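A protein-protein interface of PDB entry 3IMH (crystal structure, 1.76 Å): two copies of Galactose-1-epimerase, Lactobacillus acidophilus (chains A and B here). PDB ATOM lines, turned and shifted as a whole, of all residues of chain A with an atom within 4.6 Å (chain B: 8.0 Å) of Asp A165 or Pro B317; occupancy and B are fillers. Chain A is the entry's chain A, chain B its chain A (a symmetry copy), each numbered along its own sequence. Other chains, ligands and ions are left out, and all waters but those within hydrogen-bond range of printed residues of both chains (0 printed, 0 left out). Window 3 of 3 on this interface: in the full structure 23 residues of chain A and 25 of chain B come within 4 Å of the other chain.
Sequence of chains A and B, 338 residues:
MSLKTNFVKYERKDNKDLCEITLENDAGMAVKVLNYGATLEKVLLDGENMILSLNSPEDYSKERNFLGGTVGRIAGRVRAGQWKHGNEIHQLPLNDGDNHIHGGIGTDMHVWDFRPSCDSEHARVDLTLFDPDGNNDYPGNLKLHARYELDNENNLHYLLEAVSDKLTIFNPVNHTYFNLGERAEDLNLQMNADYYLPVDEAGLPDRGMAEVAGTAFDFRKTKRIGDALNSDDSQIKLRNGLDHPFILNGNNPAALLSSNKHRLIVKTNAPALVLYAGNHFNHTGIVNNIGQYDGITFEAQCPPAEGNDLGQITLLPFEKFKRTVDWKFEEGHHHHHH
Of the 14 printed residues of chain B, 4 touch a printed residue of chain A. Along chain B the printed residues that touch a printed residue of chain A span positions 167 to 318. Of the 8 printed residues of chain A, 4 touch a printed residue of chain B. Printed residues of chain A that touch a printed residue of chain B: Asn A141, Val A163, Asp A165 and Phe A318. Hydrophobic or aromatic side chains of chain A that line the printed part of chain B: Val A163 and Phe A318. Among the printed residues, no Asp or Glu carboxylate lies within 4 Å of a Lys or Arg side-chain nitrogen of the other chain.
Of the printed residues of chain B, Val A163 touches Leu B316. No residue of chain B comes within 4 Å of Ser A164. Of chain B, only Pro B317 (3.9 Å) comes within 4 Å of Asp A165. Of the printed residues of chain B, Phe A318 touches Pro B317 and Phe B318. Printed residues of chain A within 4 Å of Leu B167: Asn A141. Of the printed residues of chain A, Pro B317 touches Asp A165 and Phe A318. Of the printed residues of chain A, Phe B318 touches Phe A318 (3.6 Å). The nearest residue of chain B that does not touch Asp A165 is Leu B316 (4.02 Å).
Among the printed residues, pairs that only touch across the chains: Val A163 with Leu B316, Phe A318 with Pro B317, Phe A318 with Phe B318, Asn A141 with Leu B316, Asn A141 with Leu B167 and Asp A165 with Pro B317.
Asp A165 touches Pro B317, but with the chains exchanged Pro A317 does not touch Asp B165 (11.0 Å). Phe A318 touches Pro B317, but with the chains exchanged Pro A317 does not touch Phe B318 (7.4 Å). Phe B318 touches its own counterpart, Phe A318. Of the 6 pairs that touch across the chains among the printed residues, 1 has its exchanged pair printed and touching as well.
OD2 of Asp A165 lies within hydrogen-bond range of ND2 of Asn A141, 2.8 Å away. O of Ser A164 lies within hydrogen-bond range of N of Phe A318, at 2.8 Å. The backbone carbonyl oxygen of Ser B164 is in hydrogen-bond range of the backbone NH of Phe B318, 2.8 Å away. N of Leu B316 is in hydrogen-bond range of OE1 of Glu B319.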
ATOM      1  N   GLY A 140     -15.580  -5.361   5.577  1.00  0.00           N
ATOM      2  CA  GLY A 140     -14.961  -5.313   4.261  1.00  0.00           C
ATOM      3  C   GLY A 140     -13.595  -5.951   4.213  1.00  0.00           C
ATOM      4  O   GLY A 140     -12.754  -5.695   5.075  1.00  0.00           O
ATOM      5  N   ASN A 141     -13.390  -6.833   3.230  1.00  0.00           N
ATOM      6  CA  ASN A 141     -12.038  -7.254   2.867  1.00  0.00           C
ATOM      7  C   ASN A 141     -11.369  -6.033   2.287  1.00  0.00           C
ATOM      8  O   ASN A 141     -11.958  -5.340   1.465  1.00  0.00           O
ATOM      9  CB  ASN A 141     -12.082  -8.368   1.819  1.00  0.00           C
ATOM     10  CG  ASN A 141     -12.701  -9.640   2.366  1.00  0.00           C
ATOM     11  OD1 ASN A 141     -12.210 -10.209   3.348  1.00  0.00           O
ATOM     12  ND2 ASN A 141     -13.798 -10.070   1.762  1.00  0.00           N
ATOM     13  N   VAL A 163      -8.729  -0.266  -1.161  1.00  0.00           N
ATOM     14  CA  VAL A 163     -10.077  -0.571  -1.649  1.00  0.00           C
ATOM     15  C   VAL A 163     -10.701  -1.613  -0.722  1.00  0.00           C
ATOM     16  O   VAL A 163     -10.019  -2.557  -0.325  1.00  0.00           O
ATOM     17  CB  VAL A 163     -10.047  -1.182  -3.074  1.00  0.00           C
ATOM     18  CG1 VAL A 163     -11.467  -1.411  -3.601  1.00  0.00           C
ATOM     19  CG2 VAL A 163      -9.269  -0.300  -4.053  1.00  0.00           C
ATOM     20  N   SER A 164     -11.984  -1.443  -0.426  1.00  0.00           N
ATOM     21  CA  SER A 164     -12.765  -2.394   0.352  1.00  0.00           C
ATOM     22  C   SER A 164     -13.870  -3.004  -0.519  1.00  0.00           C
ATOM     23  O   SER A 164     -14.400  -2.329  -1.406  1.00  0.00           O
ATOM     24  CB  SER A 164     -13.405  -1.651   1.513  1.00  0.00           C
ATOM     25  OG  SER A 164     -14.290  -2.492   2.257  1.00  0.00           O
ATOM     26  N   ASP A 165     -14.248  -4.253  -0.242  1.00  0.00           N
ATOM     27  CA  ASP A 165     -15.414  -4.838  -0.923  1.00  0.00           C
ATOM     28  C   ASP A 165     -16.763  -4.640  -0.178  1.00  0.00           C
ATOM     29  O   ASP A 165     -17.788  -5.214  -0.573  1.00  0.00           O
ATOM     30  CB  ASP A 165     -15.179  -6.306  -1.321  1.00  0.00           C
ATOM     31  CG  ASP A 165     -15.027  -7.244  -0.121  1.00  0.00           C
ATOM     32  OD1 ASP A 165     -15.207  -6.820   1.046  1.00  0.00           O
ATOM     33  OD2 ASP A 165     -14.741  -8.443  -0.364  1.00  0.00           O
ATOM     34  N   LYS A 166     -16.754  -3.827   0.885  1.00  0.00           N
ATOM     35  CA  LYS A 166     -17.980  -3.491   1.622  1.00  0.00           C
ATOM     36  C   LYS A 166     -17.942  -2.032   2.042  1.00  0.00           C
ATOM     37  O   LYS A 166     -16.858  -1.466   2.237  1.00  0.00           O
ATOM     38  CB  LYS A 166     -18.108  -4.324   2.894  1.00  0.00           C
ATOM     39  CG  LYS A 166     -18.697  -5.710   2.723  1.00  0.00           C
ATOM     40  CD  LYS A 166     -18.988  -6.351   4.102  1.00  0.00           C
ATOM     41  CE  LYS A 166     -20.176  -5.696   4.830  1.00  0.00           C
ATOM     42  NZ  LYS A 166     -20.679  -6.515   5.987  1.00  0.00           N
ATOM     43  N   PRO A 317     -18.266   0.319  -1.317  1.00  0.00           N
ATOM     44  CA  PRO A 317     -17.548  -0.833  -1.878  1.00  0.00           C
ATOM     45  C   PRO A 317     -16.887  -0.404  -3.193  1.00  0.00           C
ATOM     46  O   PRO A 317     -17.496   0.341  -3.990  1.00  0.00           O
ATOM     47  CB  PRO A 317     -18.666  -1.846  -2.190  1.00  0.00           C
ATOM     48  CG  PRO A 317     -19.820  -1.444  -1.394  1.00  0.00           C
ATOM     49  CD  PRO A 317     -19.705   0.042  -1.113  1.00  0.00           C
ATOM     50  N   PHE A 318     -15.633  -0.823  -3.366  1.00  0.00           N
ATOM     51  CA  PHE A 318     -14.832  -0.644  -4.603  1.00  0.00           C
ATOM     52  C   PHE A 318     -14.356   0.772  -4.862  1.00  0.00           C
ATOM     53  O   PHE A 318     -13.746   1.049  -5.893  1.00  0.00           O
ATOM     54  CB  PHE A 318     -15.544  -1.265  -5.824  1.00  0.00           C
ATOM     55  CG  PHE A 318     -16.132  -2.602  -5.512  1.00  0.00           C
ATOM     56  CD1 PHE A 318     -15.309  -3.638  -5.068  1.00  0.00           C
ATOM     57  CD2 PHE A 318     -17.506  -2.806  -5.564  1.00  0.00           C
ATOM     58  CE1 PHE A 318     -15.855  -4.875  -4.710  1.00  0.00           C
ATOM     59  CE2 PHE A 318     -18.054  -4.038  -5.216  1.00  0.00           C
ATOM     60  CZ  PHE A 318     -17.217  -5.074  -4.789  1.00  0.00           C
ATOM     61  N   ASN B 141     -16.031 -15.870 -11.389  1.00  0.00           N
ATOM     62  CA  ASN B 141     -15.916 -15.807 -12.845  1.00  0.00           C
ATOM     63  C   ASN B 141     -14.735 -14.912 -13.124  1.00  0.00           C
ATOM     64  O   ASN B 141     -14.612 -13.850 -12.526  1.00  0.00           O
ATOM     65  CB  ASN B 141     -17.181 -15.205 -13.462  1.00  0.00           C
ATOM     66  CG  ASN B 141     -18.392 -16.092 -13.253  1.00  0.00           C
ATOM     67  OD1 ASN B 141     -18.407 -17.253 -13.681  1.00  0.00           O
ATOM     68  ND2 ASN B 141     -19.397 -15.568 -12.567  1.00  0.00           N
ATOM     69  N   VAL B 163      -9.569  -9.973 -14.141  1.00  0.00           N
ATOM     70  CA  VAL B 163     -10.541  -9.490 -13.156  1.00  0.00           C
ATOM     71  C   VAL B 163     -11.455 -10.652 -12.770  1.00  0.00           C
ATOM     72  O   VAL B 163     -11.870 -11.413 -13.644  1.00  0.00           O
ATOM     73  CB  VAL B 163     -11.441  -8.371 -13.739  1.00  0.00           C
ATOM     74  CG1 VAL B 163     -12.389  -7.817 -12.670  1.00  0.00           C
ATOM     75  CG2 VAL B 163     -10.616  -7.229 -14.336  1.00  0.00           C
ATOM     76  N   SER B 164     -11.775 -10.745 -11.486  1.00  0.00           N
ATOM     77  CA  SER B 164     -12.718 -11.722 -10.959  1.00  0.00           C
ATOM     78  C   SER B 164     -13.952 -11.009 -10.393  1.00  0.00           C
ATOM     79  O   SER B 164     -13.838  -9.898  -9.870  1.00  0.00           O
ATOM     80  CB  SER B 164     -12.037 -12.489  -9.839  1.00  0.00           C
ATOM     81  OG  SER B 164     -12.937 -13.386  -9.186  1.00  0.00           O
ATOM     82  N   ASP B 165     -15.117 -11.659 -10.456  1.00  0.00           N
ATOM     83  CA  ASP B 165     -16.303 -11.109  -9.783  1.00  0.00           C
ATOM     84  C   ASP B 165     -16.507 -11.606  -8.324  1.00  0.00           C
ATOM     85  O   ASP B 165     -17.547 -11.335  -7.708  1.00  0.00           O
ATOM     86  CB  ASP B 165     -17.577 -11.263 -10.633  1.00  0.00           C
ATOM     87  CG  ASP B 165     -17.995 -12.721 -10.842  1.00  0.00           C
ATOM     88  OD1 ASP B 165     -17.389 -13.648 -10.253  1.00  0.00           O
ATOM     89  OD2 ASP B 165     -18.974 -12.932 -11.602  1.00  0.00           O
ATOM     90  N   LYS B 166     -15.514 -12.322  -7.785  1.00  0.00           N
ATOM     91  CA  LYS B 166     -15.547 -12.776  -6.388  1.00  0.00           C
ATOM     92  C   LYS B 166     -14.159 -12.672  -5.781  1.00  0.00           C
ATOM     93  O   LYS B 166     -13.154 -12.767  -6.499  1.00  0.00           O
ATOM     94  CB  LYS B 166     -15.976 -14.238  -6.290  1.00  0.00           C
ATOM     95  CG  LYS B 166     -17.469 -14.495  -6.316  1.00  0.00           C
ATOM     96  CD  LYS B 166     -17.771 -15.975  -5.976  1.00  0.00           C
ATOM     97  CE  LYS B 166     -17.516 -16.315  -4.497  1.00  0.00           C
ATOM     98  NZ  LYS B 166     -18.123 -17.628  -4.083  1.00  0.00           N
ATOM     99  N   LEU B 167     -14.109 -12.468  -4.465  1.00  0.00           N
ATOM    100  CA  LEU B 167     -12.862 -12.588  -3.720  1.00  0.00           C
ATOM    101  C   LEU B 167     -12.179 -13.909  -4.113  1.00  0.00           C
ATOM    102  O   LEU B 167     -12.804 -14.979  -4.069  1.00  0.00           O
ATOM    103  CB  LEU B 167     -13.147 -12.575  -2.217  1.00  0.00           C
ATOM    104  CG  LEU B 167     -11.896 -12.580  -1.339  1.00  0.00           C
ATOM    105  CD1 LEU B 167     -11.234 -11.196  -1.307  1.00  0.00           C
ATOM    106  CD2 LEU B 167     -12.256 -13.040   0.064  1.00  0.00           C
ATOM    107  N   THR B 168     -10.915 -13.834  -4.521  1.00  0.00           N
ATOM    108  CA  THR B 168     -10.270 -15.025  -5.067  1.00  0.00           C
ATOM    109  C   THR B 168      -8.743 -14.922  -4.981  1.00  0.00           C
ATOM    110  O   THR B 168      -8.211 -13.939  -4.447  1.00  0.00           O
ATOM    111  CB  THR B 168     -10.741 -15.268  -6.531  1.00  0.00           C
ATOM    112  OG1 THR B 168     -10.421 -16.611  -6.925  1.00  0.00           O
ATOM    113  CG2 THR B 168     -10.114 -14.235  -7.494  1.00  0.00           C
ATOM    114  N   THR B 314      -4.210 -12.422  -3.347  1.00  0.00           N
ATOM    115  CA  THR B 314      -5.652 -12.320  -3.177  1.00  0.00           C
ATOM    116  C   THR B 314      -6.147 -11.140  -4.007  1.00  0.00           C
ATOM    117  O   THR B 314      -5.522 -10.093  -4.027  1.00  0.00           O
ATOM    118  CB  THR B 314      -6.001 -12.157  -1.681  1.00  0.00           C
ATOM    119  OG1 THR B 314      -5.559 -13.324  -0.972  1.00  0.00           O
ATOM    120  CG2 THR B 314      -7.512 -11.992  -1.471  1.00  0.00           C
ATOM    121  N   LEU B 315      -7.252 -11.323  -4.712  1.00  0.00           N
ATOM    122  CA  LEU B 315      -7.903 -10.235  -5.436  1.00  0.00           C
ATOM    123  C   LEU B 315      -9.290 -10.004  -4.851  1.00  0.00           C
ATOM    124  O   LEU B 315     -10.043 -10.962  -4.642  1.00  0.00           O
ATOM    125  CB  LEU B 315      -8.062 -10.608  -6.914  1.00  0.00           C
ATOM    126  CG  LEU B 315      -6.822 -10.781  -7.797  1.00  0.00           C
ATOM    127  CD1 LEU B 315      -7.269 -11.241  -9.189  1.00  0.00           C
ATOM    128  CD2 LEU B 315      -6.033  -9.474  -7.877  1.00  0.00           C
ATOM    129  N   LEU B 316      -9.621  -8.743  -4.587  1.00  0.00           N
ATOM    130  CA  LEU B 316     -11.005  -8.363  -4.287  1.00  0.00           C
ATOM    131  C   LEU B 316     -11.853  -8.551  -5.547  1.00  0.00           C
ATOM    132  O   LEU B 316     -11.307  -8.545  -6.658  1.00  0.00           O
ATOM    133  CB  LEU B 316     -11.068  -6.890  -3.874  1.00  0.00           C
ATOM    134  CG  LEU B 316     -10.374  -6.463  -2.583  1.00  0.00           C
ATOM    135  CD1 LEU B 316     -10.857  -5.068  -2.248  1.00  0.00           C
ATOM    136  CD2 LEU B 316     -10.657  -7.384  -1.435  1.00  0.00           C
ATOM    137  N   PRO B 317     -13.182  -8.698  -5.388  1.00  0.00           N
ATOM    138  CA  PRO B 317     -14.021  -8.637  -6.592  1.00  0.00           C
ATOM    139  C   PRO B 317     -13.725  -7.327  -7.329  1.00  0.00           C
ATOM    140  O   PRO B 317     -13.559  -6.267  -6.686  1.00  0.00           O
ATOM    141  CB  PRO B 317     -15.456  -8.584  -6.036  1.00  0.00           C
ATOM    142  CG  PRO B 317     -15.386  -9.078  -4.665  1.00  0.00           C
ATOM    143  CD  PRO B 317     -13.980  -8.842  -4.150  1.00  0.00           C
ATOM    144  N   PHE B 318     -13.599  -7.430  -8.653  1.00  0.00           N
ATOM    145  CA  PHE B 318     -13.437  -6.291  -9.590  1.00  0.00           C
ATOM    146  C   PHE B 318     -12.083  -5.611  -9.550  1.00  0.00           C
ATOM    147  O   PHE B 318     -11.863  -4.612 -10.232  1.00  0.00           O
ATOM    148  CB  PHE B 318     -14.610  -5.293  -9.463  1.00  0.00           C
ATOM    149  CG  PHE B 318     -15.928  -5.986  -9.361  1.00  0.00           C
ATOM    150  CD1 PHE B 318     -16.349  -6.836 -10.384  1.00  0.00           C
ATOM    151  CD2 PHE B 318     -16.705  -5.873  -8.213  1.00  0.00           C
ATOM    152  CE1 PHE B 318     -17.552  -7.540 -10.272  1.00  0.00           C
ATOM    153  CE2 PHE B 318     -17.908  -6.567  -8.101  1.00  0.00           C
ATOM    154  CZ  PHE B 318     -18.328  -7.402  -9.140  1.00  0.00           C
ATOM    155  N   GLU B 319     -11.166  -6.180  -8.772  1.00  0.00           N
ATOM    156  CA  GLU B 319      -9.794  -5.675  -8.715  1.00  0.00           C
ATOM    157  C   GLU B 319      -9.029  -6.137  -9.948  1.00  0.00           C
ATOM    158  O   GLU B 319      -9.071  -7.320 -10.311  1.00  0.00           O
ATOM    159  CB  GLU B 319      -9.087  -6.161  -7.447  1.00  0.00           C
ATOM    160  CG  GLU B 319      -7.618  -5.744  -7.383  1.00  0.00           C
ATOM    161  CD  GLU B 319      -6.882  -6.217  -6.148  1.00  0.00           C
ATOM    162  OE1 GLU B 319      -7.502  -6.745  -5.203  1.00  0.00           O
ATOM    163  OE2 GLU B 319      -5.642  -6.050  -6.136  1.00  0.00           O
ATOM    164  N   LYS B 320      -8.325  -5.197 -10.579  1.00  0.00           N
ATOM    165  CA  LYS B 320      -7.557  -5.476 -11.781  1.00  0.00           C
ATOM    166  C   LYS B 320      -6.184  -6.027 -11.419  1.00  0.00           C
ATOM    167  O   LYS B 320      -5.397  -5.358 -10.743  1.00  0.00           O
ATOM    168  CB  LYS B 320      -7.409  -4.192 -12.599  1.00  0.00           C
ATOM    169  CG  LYS B 320      -8.723  -3.683 -13.197  1.00  0.00           C
ATOM    170  CD  LYS B 320      -8.560  -2.286 -13.800  1.00  0.00           C
ATOM    171  CE  LYS B 320      -9.876  -1.796 -14.396  1.00  0.00           C
ATOM    172  NZ  LYS B 320      -9.713  -0.478 -15.070  1.00  0.00           N
